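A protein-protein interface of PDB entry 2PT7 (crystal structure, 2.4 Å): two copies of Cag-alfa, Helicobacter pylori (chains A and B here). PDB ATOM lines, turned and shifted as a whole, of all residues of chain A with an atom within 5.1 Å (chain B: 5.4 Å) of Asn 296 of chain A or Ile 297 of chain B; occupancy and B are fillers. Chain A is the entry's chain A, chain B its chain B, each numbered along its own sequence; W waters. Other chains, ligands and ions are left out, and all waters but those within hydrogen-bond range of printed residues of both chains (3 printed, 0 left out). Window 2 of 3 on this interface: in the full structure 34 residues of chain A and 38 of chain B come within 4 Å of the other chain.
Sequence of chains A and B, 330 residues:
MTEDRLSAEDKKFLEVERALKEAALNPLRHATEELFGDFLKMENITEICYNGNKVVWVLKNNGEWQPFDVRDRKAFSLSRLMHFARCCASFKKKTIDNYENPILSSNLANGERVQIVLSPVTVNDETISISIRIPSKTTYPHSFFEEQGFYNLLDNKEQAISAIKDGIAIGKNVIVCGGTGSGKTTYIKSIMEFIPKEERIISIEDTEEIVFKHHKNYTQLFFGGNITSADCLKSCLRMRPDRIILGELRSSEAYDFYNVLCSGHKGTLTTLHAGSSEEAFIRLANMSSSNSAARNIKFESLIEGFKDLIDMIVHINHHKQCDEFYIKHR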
ATOM      1  N   ALA A 293      25.602  14.891  14.484  1.00  0.00           N
ATOM      2  CA  ALA A 293      25.081  15.151  13.153  1.00  0.00           C
ATOM      3  C   ALA A 293      26.120  14.921  12.066  1.00  0.00           C
ATOM      4  O   ALA A 293      25.757  14.657  10.917  1.00  0.00           O
ATOM      5  CB  ALA A 293      24.519  16.582  13.063  1.00  0.00           C
ATOM      6  N   ALA A 294      27.401  15.010  12.437  1.00  0.00           N
ATOM      7  CA  ALA A 294      28.513  14.956  11.476  1.00  0.00           C
ATOM      8  C   ALA A 294      29.217  13.596  11.377  1.00  0.00           C
ATOM      9  O   ALA A 294      30.147  13.433  10.586  1.00  0.00           O
ATOM     10  CB  ALA A 294      29.525  16.063  11.770  1.00  0.00           C
ATOM     11  N   ARG A 295      28.761  12.620  12.154  1.00  0.00           N
ATOM     12  CA  ARG A 295      29.389  11.296  12.178  1.00  0.00           C
ATOM     13  C   ARG A 295      29.435  10.551  10.839  1.00  0.00           C
ATOM     14  O   ARG A 295      30.337   9.749  10.614  1.00  0.00           O
ATOM     15  CB  ARG A 295      28.767  10.421  13.272  1.00  0.00           C
ATOM     16  CG  ARG A 295      29.120  10.895  14.687  1.00  0.00           C
ATOM     17  CD  ARG A 295      30.650  10.990  14.885  1.00  0.00           C
ATOM     18  NE  ARG A 295      31.043  11.306  16.261  1.00  0.00           N
ATOM     19  CZ  ARG A 295      31.119  10.414  17.249  1.00  0.00           C
ATOM     20  NH1 ARG A 295      30.817   9.135  17.026  1.00  0.00           N
ATOM     21  NH2 ARG A 295      31.494  10.802  18.465  1.00  0.00           N
ATOM     22  N   ASN A 296      28.472  10.830   9.958  1.00  0.00           N
ATOM     23  CA  ASN A 296      28.431  10.222   8.628  1.00  0.00           C
ATOM     24  C   ASN A 296      28.678  11.228   7.495  1.00  0.00           C
ATOM     25  O   ASN A 296      28.208  11.032   6.376  1.00  0.00           O
ATOM     26  CB  ASN A 296      27.100   9.478   8.408  1.00  0.00           C
ATOM     27  CG  ASN A 296      26.904   8.309   9.366  1.00  0.00           C
ATOM     28  OD1 ASN A 296      27.725   7.396   9.431  1.00  0.00           O
ATOM     29  ND2 ASN A 296      25.809   8.331  10.105  1.00  0.00           N
ATOM     30  N   ILE A 297      29.425  12.292   7.784  1.00  0.00           N
ATOM     31  CA  ILE A 297      29.717  13.337   6.793  1.00  0.00           C
ATOM     32  C   ILE A 297      31.160  13.235   6.313  1.00  0.00           C
ATOM     33  O   ILE A 297      32.068  13.147   7.123  1.00  0.00           O
ATOM     34  CB  ILE A 297      29.432  14.771   7.355  1.00  0.00           C
ATOM     35  CG1 ILE A 297      27.973  14.891   7.810  1.00  0.00           C
ATOM     36  CG2 ILE A 297      29.764  15.850   6.307  1.00  0.00           C
ATOM     37  CD1 ILE A 297      27.531  16.281   8.226  1.00  0.00           C
ATOM     38  N   LYS A 298      31.360  13.245   4.997  1.00  0.00           N
ATOM     39  CA  LYS A 298      32.695  13.251   4.410  1.00  0.00           C
ATOM     40  C   LYS A 298      33.486  14.486   4.853  1.00  0.00           C
ATOM     41  O   LYS A 298      32.994  15.620   4.760  1.00  0.00           O
ATOM     42  CB  LYS A 298      32.622  13.238   2.886  1.00  0.00           C
ATOM     43  CG  LYS A 298      31.980  12.006   2.272  1.00  0.00           C
ATOM     44  CD  LYS A 298      31.902  12.180   0.766  1.00  0.00           C
ATOM     45  CE  LYS A 298      31.048  11.116   0.118  1.00  0.00           C
ATOM     46  NZ  LYS A 298      30.571  11.540  -1.233  1.00  0.00           N
ATOM     47  N   TYR B 255      13.514  14.218  10.844  1.00  0.00           N
ATOM     48  CA  TYR B 255      13.532  12.855  10.348  1.00  0.00           C
ATOM     49  C   TYR B 255      12.110  12.288  10.286  1.00  0.00           C
ATOM     50  O   TYR B 255      11.754  11.603   9.334  1.00  0.00           O
ATOM     51  CB  TYR B 255      14.451  11.986  11.208  1.00  0.00           C
ATOM     52  CG  TYR B 255      14.542  10.549  10.742  1.00  0.00           C
ATOM     53  CD1 TYR B 255      15.353  10.194   9.664  1.00  0.00           C
ATOM     54  CD2 TYR B 255      13.812   9.543  11.376  1.00  0.00           C
ATOM     55  CE1 TYR B 255      15.431   8.874   9.228  1.00  0.00           C
ATOM     56  CE2 TYR B 255      13.883   8.225  10.952  1.00  0.00           C
ATOM     57  CZ  TYR B 255      14.696   7.895   9.879  1.00  0.00           C
ATOM     58  OH  TYR B 255      14.770   6.578   9.461  1.00  0.00           O
ATOM     59  N   ALA B 293      17.468   7.140  14.797  1.00  0.00           N
ATOM     60  CA  ALA B 293      17.052   6.266  13.692  1.00  0.00           C
ATOM     61  C   ALA B 293      17.836   6.508  12.396  1.00  0.00           C
ATOM     62  O   ALA B 293      17.751   5.715  11.445  1.00  0.00           O
ATOM     63  CB  ALA B 293      15.562   6.418  13.437  1.00  0.00           C
ATOM     64  N   ALA B 294      18.602   7.600  12.375  1.00  0.00           N
ATOM     65  CA  ALA B 294      19.399   7.987  11.214  1.00  0.00           C
ATOM     66  C   ALA B 294      20.912   7.844  11.423  1.00  0.00           C
ATOM     67  O   ALA B 294      21.697   8.323  10.604  1.00  0.00           O
ATOM     68  CB  ALA B 294      19.052   9.410  10.807  1.00  0.00           C
ATOM     69  N   ARG B 295      21.317   7.171  12.501  1.00  0.00           N
ATOM     70  CA  ARG B 295      22.727   7.139  12.900  1.00  0.00           C
ATOM     71  C   ARG B 295      23.659   6.368  11.960  1.00  0.00           C
ATOM     72  O   ARG B 295      24.878   6.561  12.002  1.00  0.00           O
ATOM     73  CB  ARG B 295      22.897   6.663  14.355  1.00  0.00           C
ATOM     74  CG  ARG B 295      22.631   5.189  14.602  1.00  0.00           C
ATOM     75  CD  ARG B 295      23.604   4.643  15.641  1.00  0.00           C
ATOM     76  NE  ARG B 295      23.308   3.252  15.991  1.00  0.00           N
ATOM     77  CZ  ARG B 295      22.528   2.879  17.004  1.00  0.00           C
ATOM     78  NH1 ARG B 295      21.953   3.791  17.788  1.00  0.00           N
ATOM     79  NH2 ARG B 295      22.320   1.588  17.236  1.00  0.00           N
ATOM     80  N   ASN B 296      23.087   5.501  11.125  1.00  0.00           N
ATOM     81  CA  ASN B 296      23.860   4.733  10.146  1.00  0.00           C
ATOM     82  C   ASN B 296      23.445   4.998   8.702  1.00  0.00           C
ATOM     83  O   ASN B 296      23.684   4.173   7.812  1.00  0.00           O
ATOM     84  CB  ASN B 296      23.788   3.241  10.457  1.00  0.00           C
ATOM     85  CG  ASN B 296      24.625   2.860  11.653  1.00  0.00           C
ATOM     86  OD1 ASN B 296      25.844   3.051  11.660  1.00  0.00           O
ATOM     87  ND2 ASN B 296      23.981   2.306  12.672  1.00  0.00           N
ATOM     88  N   ILE B 297      22.827   6.157   8.484  1.00  0.00           N
ATOM     89  CA  ILE B 297      22.439   6.610   7.154  1.00  0.00           C
ATOM     90  C   ILE B 297      23.421   7.677   6.677  1.00  0.00           C
ATOM     91  O   ILE B 297      23.716   8.628   7.402  1.00  0.00           O
ATOM     92  CB  ILE B 297      20.993   7.195   7.126  1.00  0.00           C
ATOM     93  CG1 ILE B 297      19.980   6.210   7.733  1.00  0.00           C
ATOM     94  CG2 ILE B 297      20.602   7.604   5.703  1.00  0.00           C
ATOM     95  CD1 ILE B 297      18.569   6.802   7.946  1.00  0.00           C
ATOM     96  N   LYS B 298      23.911   7.508   5.450  1.00  0.00           N
ATOM     97  CA  LYS B 298      24.797   8.477   4.809  1.00  0.00           C
ATOM     98  C   LYS B 298      24.148   9.843   4.733  1.00  0.00           C
ATOM     99  O   LYS B 298      22.975   9.968   4.383  1.00  0.00           O
ATOM    100  CB  LYS B 298      25.176   8.030   3.399  1.00  0.00           C
ATOM    101  CG  LYS B 298      25.998   6.747   3.331  1.00  0.00           C
ATOM    102  CD  LYS B 298      26.550   6.531   1.928  1.00  0.00           C
ATOM    103  CE  LYS B 298      25.452   6.194   0.927  1.00  0.00           C
ATOM    104  NZ  LYS B 298      24.903   4.816   1.155  1.00  0.00           N
ATOM    105  N   PHE B 299      24.924  10.869   5.060  1.00  0.00           N
ATOM    106  CA  PHE B 299      24.467  12.235   4.977  1.00  0.00           C
ATOM    107  C   PHE B 299      23.955  12.599   3.571  1.00  0.00           C
ATOM    108  O   PHE B 299      23.022  13.394   3.436  1.00  0.00           O
ATOM    109  CB  PHE B 299      25.587  13.174   5.396  1.00  0.00           C
ATOM    110  CG  PHE B 299      25.179  14.617   5.427  1.00  0.00           C
ATOM    111  CD1 PHE B 299      24.508  15.135   6.526  1.00  0.00           C
ATOM    112  CD2 PHE B 299      25.464  15.456   4.357  1.00  0.00           C
ATOM    113  CE1 PHE B 299      24.131  16.474   6.567  1.00  0.00           C
ATOM    114  CE2 PHE B 299      25.086  16.802   4.392  1.00  0.00           C
ATOM    115  CZ  PHE B 299      24.418  17.305   5.500  1.00  0.00           C
ATOM    116  N   GLU B 300      24.590  12.024   2.545  1.00  0.00           N
ATOM    117  CA  GLU B 300      24.219  12.203   1.145  1.00  0.00           C
ATOM    118  C   GLU B 300      22.800  11.714   0.873  1.00  0.00           C
ATOM    119  O   GLU B 300      22.023  12.381   0.186  1.00  0.00           O
ATOM    120  CB  GLU B 300      25.177  11.420   0.230  1.00  0.00           C
ATOM    121  CG  GLU B 300      26.652  11.792   0.340  1.00  0.00           C
ATOM    122  CD  GLU B 300      27.509  10.643   0.883  1.00  0.00           C
ATOM    123  OE1 GLU B 300      27.659  10.558   2.173  1.00  0.00           O
ATOM    124  OE2 GLU B 300      28.065   9.804   0.073  1.00  0.00           O
ATOM    125  N   SER B 301      22.484  10.530   1.402  1.00  0.00           N
ATOM    126  CA  SER B 301      21.168   9.909   1.263  1.00  0.00           C
ATOM    127  C   SER B 301      20.081  10.730   1.942  1.00  0.00           C
ATOM    128  O   SER B 301      18.957  10.793   1.453  1.00  0.00           O
ATOM    129  CB  SER B 301      21.198   8.516   1.876  1.00  0.00           C
ATOM    130  OG  SER B 301      22.300   7.786   1.378  1.00  0.00           O
ATOM    131  N   LEU B 302      20.405  11.344   3.076  1.00  0.00           N
ATOM    132  CA  LEU B 302      19.466  12.246   3.750  1.00  0.00           C
ATOM    133  C   LEU B 302      19.140  13.475   2.898  1.00  0.00           C
ATOM    134  O   LEU B 302      17.965  13.792   2.686  1.00  0.00           O
ATOM    135  CB  LEU B 302      19.987  12.667   5.125  1.00  0.00           C
ATOM    136  CG  LEU B 302      20.192  11.525   6.128  1.00  0.00           C
ATOM    137  CD1 LEU B 302      20.960  12.030   7.327  1.00  0.00           C
ATOM    138  CD2 LEU B 302      18.864  10.865   6.553  1.00  0.00           C
HETATM  139  O   HOH W   1      28.736  13.452   3.023  1.00  0.00           O
HETATM  140  O   HOH W   2      28.222   9.442   4.470  1.00  0.00           O
HETATM  141  O   HOH W   3      23.341  10.068   9.600  1.00  0.00           O
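The side-chain amide nitrogen (ND2) of Asn 296 of chain A is in hydrogen-bond range of the backbone carbonyl oxygen (O) of Arg 295 of chain B (2.8 Å). The backbone carbonyl oxygen (O) of Ile 297 of chain B lies within hydrogen-bond range of the side-chain amide nitrogen (ND2) of Asn 296 of chain A (3.4 Å). The side-chain carboxylate (OE2) of Glu 300 of chain B lies within salt-bridge range of the side-chain amino group (NZ) of Lys 298 of chain A (3.3 Å).
Asn 296 of chain A touches Phe 299 of chain B. Phe 299 of chain B touches Ile 297 of chain A.
Asn 296 of chain A touches three residues of chain B. Ile 297 of chain B touches just one residue of chain A: Asn 296. Printed residues of chain A within 4 Å of Arg 295 of chain B: Asn 296 (2.8 Å). Of the printed residues of chain A, Phe 299 of chain B touches Asn 296 (3.5 Å) and Ile 297 (3.7 Å). Of the printed residues of chain A, Glu 300 of chain B touches Lys 298. Printed residues of chain B within 4 Å of Lys 298 of chain A: Glu 300 (3.3 Å). The nearest printed residue of chain A that does not touch Ile 297 of chain B is Ile 297 of chain A (6.8 Å).
Of the 6 printed residues of chain A, 3 touch a printed residue of chain B. Hydrophobic or aromatic side chains of chain A within 4 Å of the printed part of chain B: Ile 297. Of the 11 printed residues of chain B, 4 touch a printed residue of chain A. Printed residues of chain B that touch a printed residue of chain A: Arg 295, Ile 297, Phe 299 and Glu 300. Among the printed residues, Asp or Glu carboxylates within 4 Å of a Lys or Arg side-chain nitrogen of the other chain: Lys 298 of chain A with Glu 300 of chain B.
Asn 296 of chain A touches Arg 295 of chain B, but with the chains exchanged Arg 295 of chain A does not touch Asn 296 of chain B (7.8 Å). Asn 296 of chain A touches Ile 297 of chain B, but with the chains exchanged Ile 297 of chain A does not touch Asn 296 of chain B (9.5 Å). Of the 5 pairs that touch across the chains among the printed residues, none has its exchanged pair printed and touching as well.
Water W2 lies within hydrogen-bond range of O of Asn 296 of chain A and OE1 of Glu 300 of chain B. Water W3 lies within hydrogen-bond range of O of Ala 294 of chain B (2.6 Å), O of Ile 297 of chain B (2.7 Å) and ND2 of Asn 296 of chain A (3.1 Å). Water W1 lies within hydrogen-bond range of OE1 of Glu 300 of chain B (3.2 Å) and N of Lys 298 of chain A (3.3 Å).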
